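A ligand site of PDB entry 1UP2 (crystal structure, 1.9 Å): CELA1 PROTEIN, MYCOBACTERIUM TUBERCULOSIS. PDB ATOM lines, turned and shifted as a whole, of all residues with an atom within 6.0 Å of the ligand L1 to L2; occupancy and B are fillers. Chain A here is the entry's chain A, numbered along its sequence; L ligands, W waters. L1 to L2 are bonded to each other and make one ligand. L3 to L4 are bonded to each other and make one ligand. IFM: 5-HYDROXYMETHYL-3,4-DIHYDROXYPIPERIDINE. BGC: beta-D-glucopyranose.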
ATOM      1  N   TYR A  76      37.638  -7.989  19.334  1.00  0.00           N
ATOM      2  CA  TYR A  76      37.073  -9.333  19.541  1.00  0.00           C
ATOM      3  C   TYR A  76      38.161 -10.283  20.053  1.00  0.00           C
ATOM      4  O   TYR A  76      38.463 -11.297  19.416  1.00  0.00           O
ATOM      5  CB  TYR A  76      36.418  -9.827  18.238  1.00  0.00           C
ATOM      6  CG  TYR A  76      35.524 -11.022  18.359  1.00  0.00           C
ATOM      7  CD1 TYR A  76      34.540 -11.128  19.377  1.00  0.00           C
ATOM      8  CD2 TYR A  76      35.582 -12.055  17.396  1.00  0.00           C
ATOM      9  CE1 TYR A  76      33.719 -12.241  19.481  1.00  0.00           C
ATOM     10  CE2 TYR A  76      34.783 -13.198  17.534  1.00  0.00           C
ATOM     11  CZ  TYR A  76      33.852 -13.276  18.561  1.00  0.00           C
ATOM     12  OH  TYR A  76      33.032 -14.402  18.635  1.00  0.00           O
ATOM     13  N   ASP A  82      33.646 -16.399  22.709  1.00  0.00           N
ATOM     14  CA  ASP A  82      32.552 -17.239  22.221  1.00  0.00           C
ATOM     15  C   ASP A  82      32.274 -18.471  23.066  1.00  0.00           C
ATOM     16  O   ASP A  82      31.617 -19.420  22.590  1.00  0.00           O
ATOM     17  CB  ASP A  82      32.807 -17.687  20.769  1.00  0.00           C
ATOM     18  CG  ASP A  82      31.521 -17.958  20.020  1.00  0.00           C
ATOM     19  OD1 ASP A  82      30.521 -17.219  20.241  1.00  0.00           O
ATOM     20  OD2 ASP A  82      31.410 -18.896  19.212  1.00  0.00           O
ATOM     21  N   SER A  85      32.952 -21.883  21.559  1.00  0.00           N
ATOM     22  CA  SER A  85      32.096 -22.405  20.506  1.00  0.00           C
ATOM     23  C   SER A  85      32.660 -22.157  19.082  1.00  0.00           C
ATOM     24  O   SER A  85      33.877 -22.259  18.883  1.00  0.00           O
ATOM     25  CB  SER A  85      30.660 -21.932  20.691  1.00  0.00           C
ATOM     26  OG  SER A  85      29.799 -22.604  19.797  1.00  0.00           O
ATOM     27  N   ALA A  87      33.299 -19.681  17.275  1.00  0.00           N
ATOM     28  CA  ALA A  87      34.276 -18.591  17.137  1.00  0.00           C
ATOM     29  C   ALA A  87      35.247 -18.554  18.297  1.00  0.00           C
ATOM     30  O   ALA A  87      35.700 -17.479  18.708  1.00  0.00           O
ATOM     31  CB  ALA A  87      33.537 -17.227  16.962  1.00  0.00           C
ATOM     32  N   ASP A 120      29.271  -9.904  22.069  1.00  0.00           N
ATOM     33  CA  ASP A 120      28.809 -11.059  22.812  1.00  0.00           C
ATOM     34  C   ASP A 120      29.381 -11.176  24.238  1.00  0.00           C
ATOM     35  O   ASP A 120      28.866 -11.962  24.995  1.00  0.00           O
ATOM     36  CB  ASP A 120      29.064 -12.397  22.124  1.00  0.00           C
ATOM     37  CG  ASP A 120      28.515 -12.481  20.731  1.00  0.00           C
ATOM     38  OD1 ASP A 120      27.545 -11.770  20.409  1.00  0.00           O
ATOM     39  OD2 ASP A 120      29.016 -13.247  19.897  1.00  0.00           O
ATOM     40  N   MHO A 124      26.909 -13.128  26.629  1.00  0.00           N
ATOM     41  CA  MHO A 124      27.211 -14.544  26.770  1.00  0.00           C
ATOM     42  CB  MHO A 124      28.064 -14.875  25.543  1.00  0.00           C
ATOM     43  CG  MHO A 124      27.906 -16.317  25.108  1.00  0.00           C
ATOM     44  SD  MHO A 124      28.594 -16.691  23.447  1.00  0.00           S
ATOM     45  CE  MHO A 124      28.029 -18.355  23.194  1.00  0.00           C
ATOM     46  C   MHO A 124      27.947 -14.938  28.039  1.00  0.00           C
ATOM     47  O   MHO A 124      28.197 -16.127  28.233  1.00  0.00           O
ATOM     48  OD1 MHO A 124      30.149 -16.344  23.807  1.00  0.00           O
ATOM     49  N   HIS A 161      21.415  -8.349  21.979  1.00  0.00           N
ATOM     50  CA  HIS A 161      20.256  -8.039  21.144  1.00  0.00           C
ATOM     51  C   HIS A 161      18.959  -8.249  21.915  1.00  0.00           C
ATOM     52  O   HIS A 161      18.939  -8.747  23.033  1.00  0.00           O
ATOM     53  CB  HIS A 161      20.247  -8.821  19.797  1.00  0.00           C
ATOM     54  CG  HIS A 161      20.221 -10.316  19.952  1.00  0.00           C
ATOM     55  ND1 HIS A 161      19.225 -10.988  20.618  1.00  0.00           N
ATOM     56  CD2 HIS A 161      21.077 -11.263  19.491  1.00  0.00           C
ATOM     57  CE1 HIS A 161      19.487 -12.279  20.601  1.00  0.00           C
ATOM     58  NE2 HIS A 161      20.605 -12.472  19.928  1.00  0.00           N
ATOM     59  N   ARG A 163      16.592 -10.206  21.890  1.00  0.00           N
ATOM     60  CA  ARG A 163      16.132 -11.526  22.277  1.00  0.00           C
ATOM     61  C   ARG A 163      17.177 -12.343  23.026  1.00  0.00           C
ATOM     62  O   ARG A 163      17.112 -13.562  23.076  1.00  0.00           O
ATOM     63  CB  ARG A 163      15.612 -12.272  21.045  1.00  0.00           C
ATOM     64  CG  ARG A 163      14.366 -11.572  20.564  1.00  0.00           C
ATOM     65  CD  ARG A 163      13.487 -12.364  19.687  1.00  0.00           C
ATOM     66  NE  ARG A 163      12.643 -11.456  18.892  1.00  0.00           N
ATOM     67  CZ  ARG A 163      11.871 -11.897  17.894  1.00  0.00           C
ATOM     68  NH1 ARG A 163      11.795 -13.204  17.626  1.00  0.00           N
ATOM     69  NH2 ARG A 163      11.159 -11.061  17.160  1.00  0.00           N
ATOM     70  N   TRP A 164      18.101 -11.647  23.677  1.00  0.00           N
ATOM     71  CA  TRP A 164      19.143 -12.295  24.448  1.00  0.00           C
ATOM     72  C   TRP A 164      18.885 -11.982  25.938  1.00  0.00           C
ATOM     73  O   TRP A 164      17.966 -12.562  26.537  1.00  0.00           O
ATOM     74  CB  TRP A 164      20.535 -11.855  23.939  1.00  0.00           C
ATOM     75  CG  TRP A 164      21.616 -12.791  24.257  1.00  0.00           C
ATOM     76  CD1 TRP A 164      21.625 -13.712  25.265  1.00  0.00           C
ATOM     77  CD2 TRP A 164      22.885 -12.904  23.590  1.00  0.00           C
ATOM     78  NE1 TRP A 164      22.818 -14.389  25.260  1.00  0.00           N
ATOM     79  CE2 TRP A 164      23.602 -13.935  24.242  1.00  0.00           C
ATOM     80  CE3 TRP A 164      23.475 -12.276  22.489  1.00  0.00           C
ATOM     81  CZ2 TRP A 164      24.899 -14.317  23.851  1.00  0.00           C
ATOM     82  CZ3 TRP A 164      24.761 -12.640  22.107  1.00  0.00           C
ATOM     83  CH2 TRP A 164      25.460 -13.645  22.786  1.00  0.00           C
ATOM     84  N   ASN A 188      22.657  -6.068  18.051  1.00  0.00           N
ATOM     85  CA  ASN A 188      22.387  -6.884  16.851  1.00  0.00           C
ATOM     86  C   ASN A 188      23.631  -7.323  16.086  1.00  0.00           C
ATOM     87  O   ASN A 188      23.515  -7.751  14.916  1.00  0.00           O
ATOM     88  CB  ASN A 188      21.496  -6.097  15.844  1.00  0.00           C
ATOM     89  CG  ASN A 188      20.527  -7.004  15.112  1.00  0.00           C
ATOM     90  OD1 ASN A 188      20.030  -7.976  15.689  1.00  0.00           O
ATOM     91  ND2 ASN A 188      20.197  -6.667  13.862  1.00  0.00           N
ATOM     92  N   VAL A 189      24.805  -7.234  16.723  1.00  0.00           N
ATOM     93  CA  VAL A 189      26.055  -7.561  16.041  1.00  0.00           C
ATOM     94  C   VAL A 189      26.042  -9.041  15.610  1.00  0.00           C
ATOM     95  O   VAL A 189      25.880  -9.930  16.448  1.00  0.00           O
ATOM     96  CB  VAL A 189      27.311  -7.265  16.877  1.00  0.00           C
ATOM     97  CG1 VAL A 189      28.558  -7.776  16.193  1.00  0.00           C
ATOM     98  CG2 VAL A 189      27.434  -5.777  17.114  1.00  0.00           C
ATOM     99  N   SER A 190      26.184  -9.242  14.304  1.00  0.00           N
ATOM    100  CA  SER A 190      26.157 -10.532  13.639  1.00  0.00           C
ATOM    101  C   SER A 190      24.814 -11.225  13.789  1.00  0.00           C
ATOM    102  O   SER A 190      24.715 -12.416  13.559  1.00  0.00           O
ATOM    103  CB  SER A 190      27.262 -11.473  14.164  1.00  0.00           C
ATOM    104  OG  SER A 190      28.553 -10.859  14.218  1.00  0.00           O
ATOM    105  N   ASN A 191      23.785 -10.478  14.157  1.00  0.00           N
ATOM    106  CA  ASN A 191      22.450 -11.040  14.188  1.00  0.00           C
ATOM    107  C   ASN A 191      21.538 -10.405  13.115  1.00  0.00           C
ATOM    108  O   ASN A 191      22.029  -9.723  12.211  1.00  0.00           O
ATOM    109  CB  ASN A 191      21.886 -11.074  15.604  1.00  0.00           C
ATOM    110  CG  ASN A 191      21.027 -12.318  15.872  1.00  0.00           C
ATOM    111  OD1 ASN A 191      19.973 -12.516  15.214  1.00  0.00           O
ATOM    112  ND2 ASN A 191      21.461 -13.170  16.801  1.00  0.00           N
ATOM    113  N   TYR A 193      17.861  -9.383  13.764  1.00  0.00           N
ATOM    114  CA  TYR A 193      16.580  -8.796  14.220  1.00  0.00           C
ATOM    115  C   TYR A 193      16.308  -7.453  13.546  1.00  0.00           C
ATOM    116  O   TYR A 193      17.252  -6.748  13.206  1.00  0.00           O
ATOM    117  CB  TYR A 193      16.531  -8.709  15.744  1.00  0.00           C
ATOM    118  CG  TYR A 193      16.619 -10.061  16.377  1.00  0.00           C
ATOM    119  CD1 TYR A 193      15.535 -10.916  16.336  1.00  0.00           C
ATOM    120  CD2 TYR A 193      17.803 -10.525  16.950  1.00  0.00           C
ATOM    121  CE1 TYR A 193      15.599 -12.187  16.864  1.00  0.00           C
ATOM    122  CE2 TYR A 193      17.874 -11.814  17.489  1.00  0.00           C
ATOM    123  CZ  TYR A 193      16.767 -12.625  17.445  1.00  0.00           C
ATOM    124  OH  TYR A 193      16.773 -13.907  17.942  1.00  0.00           O
ATOM    125  N   ASN A 232      19.613 -20.510  14.890  1.00  0.00           N
ATOM    126  CA  ASN A 232      19.036 -19.687  13.815  1.00  0.00           C
ATOM    127  C   ASN A 232      19.890 -18.456  13.424  1.00  0.00           C
ATOM    128  O   ASN A 232      19.672 -17.840  12.377  1.00  0.00           O
ATOM    129  CB  ASN A 232      17.566 -19.292  14.105  1.00  0.00           C
ATOM    130  CG  ASN A 232      17.437 -18.222  15.157  1.00  0.00           C
ATOM    131  OD1 ASN A 232      18.282 -18.101  16.064  1.00  0.00           O
ATOM    132  ND2 ASN A 232      16.332 -17.471  15.087  1.00  0.00           N
ATOM    133  N   TRP A 233      20.862 -18.127  14.272  1.00  0.00           N
ATOM    134  CA  TRP A 233      21.843 -17.067  14.013  1.00  0.00           C
ATOM    135  C   TRP A 233      23.087 -17.619  13.267  1.00  0.00           C
ATOM    136  O   TRP A 233      23.982 -16.861  12.909  1.00  0.00           O
ATOM    137  CB  TRP A 233      22.250 -16.405  15.356  1.00  0.00           C
ATOM    138  CG  TRP A 233      22.542 -17.436  16.401  1.00  0.00           C
ATOM    139  CD1 TRP A 233      21.653 -17.941  17.320  1.00  0.00           C
ATOM    140  CD2 TRP A 233      23.736 -18.225  16.537  1.00  0.00           C
ATOM    141  NE1 TRP A 233      22.248 -18.940  18.042  1.00  0.00           N
ATOM    142  CE2 TRP A 233      23.519 -19.125  17.588  1.00  0.00           C
ATOM    143  CE3 TRP A 233      24.980 -18.199  15.918  1.00  0.00           C
ATOM    144  CZ2 TRP A 233      24.489 -20.042  18.020  1.00  0.00           C
ATOM    145  CZ3 TRP A 233      25.958 -19.089  16.351  1.00  0.00           C
ATOM    146  CH2 TRP A 233      25.694 -20.004  17.394  1.00  0.00           C
HETATM  147  O4  IFM L   1      23.835 -17.103  20.521  1.00  0.00           O
HETATM  148  C4  IFM L   1      22.845 -16.555  21.401  1.00  0.00           C
HETATM  149  C3  IFM L   1      21.630 -16.126  20.589  1.00  0.00           C
HETATM  150  O3  IFM L   1      21.969 -14.982  19.794  1.00  0.00           O
HETATM  151  C2  IFM L   1      20.436 -15.762  21.494  1.00  0.00           C
HETATM  152  N   IFM L   1      20.175 -16.779  22.506  1.00  0.00           N
HETATM  153  C1  IFM L   1      21.326 -17.174  23.318  1.00  0.00           C
HETATM  154  C5  IFM L   1      22.472 -17.642  22.414  1.00  0.00           C
HETATM  155  C6  IFM L   1      23.760 -17.966  23.209  1.00  0.00           C
HETATM  156  O6  IFM L   1      23.447 -18.860  24.264  1.00  0.00           O
HETATM  157  C2  BGC L   2      26.068 -17.007  19.685  1.00  0.00           C
HETATM  158  C3  BGC L   2      27.185 -16.060  19.255  1.00  0.00           C
HETATM  159  C4  BGC L   2      26.660 -15.062  18.200  1.00  0.00           C
HETATM  160  C5  BGC L   2      25.395 -14.372  18.700  1.00  0.00           C
HETATM  161  C6  BGC L   2      24.786 -13.465  17.620  1.00  0.00           C
HETATM  162  C1  BGC L   2      24.864 -16.198  20.136  1.00  0.00           C
HETATM  163  O2  BGC L   2      26.486 -17.967  20.641  1.00  0.00           O
HETATM  164  O3  BGC L   2      28.260 -16.809  18.702  1.00  0.00           O
HETATM  165  O4  BGC L   2      27.649 -14.092  17.901  1.00  0.00           O
HETATM  166  O5  BGC L   2      24.423 -15.351  19.064  1.00  0.00           O
HETATM  167  O6  BGC L   2      23.693 -12.780  18.210  1.00  0.00           O
HETATM  168  O4  IFM L   3      32.303 -14.448  13.691  1.00  0.00           O
HETATM  169  C4  IFM L   3      31.115 -13.944  14.334  1.00  0.00           C
HETATM  170  C3  IFM L   3      29.994 -14.802  13.791  1.00  0.00           C
HETATM  171  O3  IFM L   3      29.638 -14.336  12.486  1.00  0.00           O
HETATM  172  C2  IFM L   3      28.811 -14.859  14.745  1.00  0.00           C
HETATM  173  N   IFM L   3      29.157 -15.455  16.046  1.00  0.00           N
HETATM  174  C1  IFM L   3      30.533 -15.274  16.496  1.00  0.00           C
HETATM  175  C5  IFM L   3      31.248 -14.055  15.878  1.00  0.00           C
HETATM  176  C6  IFM L   3      30.854 -12.757  16.562  1.00  0.00           C
HETATM  177  O6  IFM L   3      29.604 -12.268  16.160  1.00  0.00           O
HETATM  178  C2  BGC L   4      34.640 -14.141  13.382  1.00  0.00           C
HETATM  179  C3  BGC L   4      35.737 -13.123  12.980  1.00  0.00           C
HETATM  180  C4  BGC L   4      35.298 -12.163  11.878  1.00  0.00           C
HETATM  181  C5  BGC L   4      33.880 -11.592  12.179  1.00  0.00           C
HETATM  182  C6  BGC L   4      33.250 -10.673  11.115  1.00  0.00           C
HETATM  183  C1  BGC L   4      33.284 -13.447  13.542  1.00  0.00           C
HETATM  184  O2  BGC L   4      34.979 -14.912  14.539  1.00  0.00           O
HETATM  185  O3  BGC L   4      36.930 -13.794  12.630  1.00  0.00           O
HETATM  186  O4  BGC L   4      36.287 -11.154  11.792  1.00  0.00           O
HETATM  187  O5  BGC L   4      32.982 -12.667  12.412  1.00  0.00           O
HETATM  188  O6  BGC L   4      32.865 -11.420   9.968  1.00  0.00           O
HETATM  189  O   HOH W   1      28.961 -19.463  18.007  1.00  0.00           O
HETATM  190  O   HOH W   2      21.956 -18.715  26.486  1.00  0.00           O
HETATM  191  O   HOH W   3      24.289 -10.100  18.640  1.00  0.00           O
HETATM  192  O   HOH W   4      23.813 -16.808  26.688  1.00  0.00           O
HETATM  193  O   HOH W   5      25.778 -20.467  21.483  1.00  0.00           O
HETATM  194  O   HOH W   6      18.532 -15.922  24.586  1.00  0.00           O
HETATM  195  O   HOH W   7      28.102 -10.842  17.915  1.00  0.00           O
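An oxygen (O4) of BGC L2 is in hydrogen-bond range of a nitrogen (N) of IFM L3, 2.8 Å away.
A ring nitrogen (ND1) of His 161 sits at hydrogen-bond distance from the backbone NH (N) of Arg 163, 3.0 Å away.
A ring nitrogen (NE2) of His 161 is in hydrogen-bond range of the side-chain amide nitrogen of Asn 191 (3.3 Å).
A ring nitrogen (ND1) of His 161 lies within hydrogen-bond range of the backbone NH (N) of Trp 164 (3.3 Å).
The side-chain carboxylate of Asp 82 is in hydrogen-bond range of the backbone NH of Ala 87 (2.8 Å).
Water W3 lies within hydrogen-bond range of O of Val 189 (2.7 Å) and O6 of BGC L2 (2.8 Å).
Water W6 lies within hydrogen-bond range of a nitrogen (N) of IFM L1 (2.8 Å) and the backbone carbonyl oxygen of Arg 163 (3.1 Å).
Water W1 bridges the side-chain carboxylate of Asp 82 (2.8 Å) and an oxygen (O3) of BGC L2 (2.8 Å).
Water W4 lies within hydrogen-bond range of the indole nitrogen (NE1) of Trp 164 and an oxygen (O6) of IFM L1.
Water W7 lies within hydrogen-bond range of O6 of IFM L3 (2.7 Å), OD1 of Asp 120 (2.7 Å), O of Val 189 (2.8 Å) and O4 of BGC L2 (3.3 Å).
An oxygen (O6) of BGC L2 sits at hydrogen-bond distance from the side-chain amide nitrogen (ND2) of Asn 191 (2.7 Å).
NE2 of His 161 sits at hydrogen-bond distance from O3 of IFM L1 (2.9 Å).
The side-chain carboxylate of Asp 82 is in hydrogen-bond range of an oxygen (O3) of BGC L2, at 2.8 Å.
The side-chain carboxylate of Asp 120 lies within hydrogen-bond range of an oxygen (O4) of BGC L2.
The side-chain hydroxyl (OG) of Ser 190 sits at hydrogen-bond distance from an oxygen (O6) of IFM L3, at 2.6 Å.
NE1 of Trp 233 sits at hydrogen-bond distance from O4 of IFM L1 (3.5 Å).
SD of MHO 124 sits close to O2 of BGC L2 (3.7 Å).
Residues that only touch the ligand L1 to L2: Trp 164 (3.7 Å) and Val 189 (3.9 Å).
Hydrophobic or aromatic side chains within 4 Å of the ligand L1 to L2: His 161, Trp 164 and Trp 233.
Within 4 Å of the ligand L1 to L2: Asp 82, Asp 120, MHO 124, His 161, Trp 164, Val 189, Asn 191 and Trp 233.
The nearest printed residue that does not touch the ligand L1 to L2 is Ser 190 (4.2 Å).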
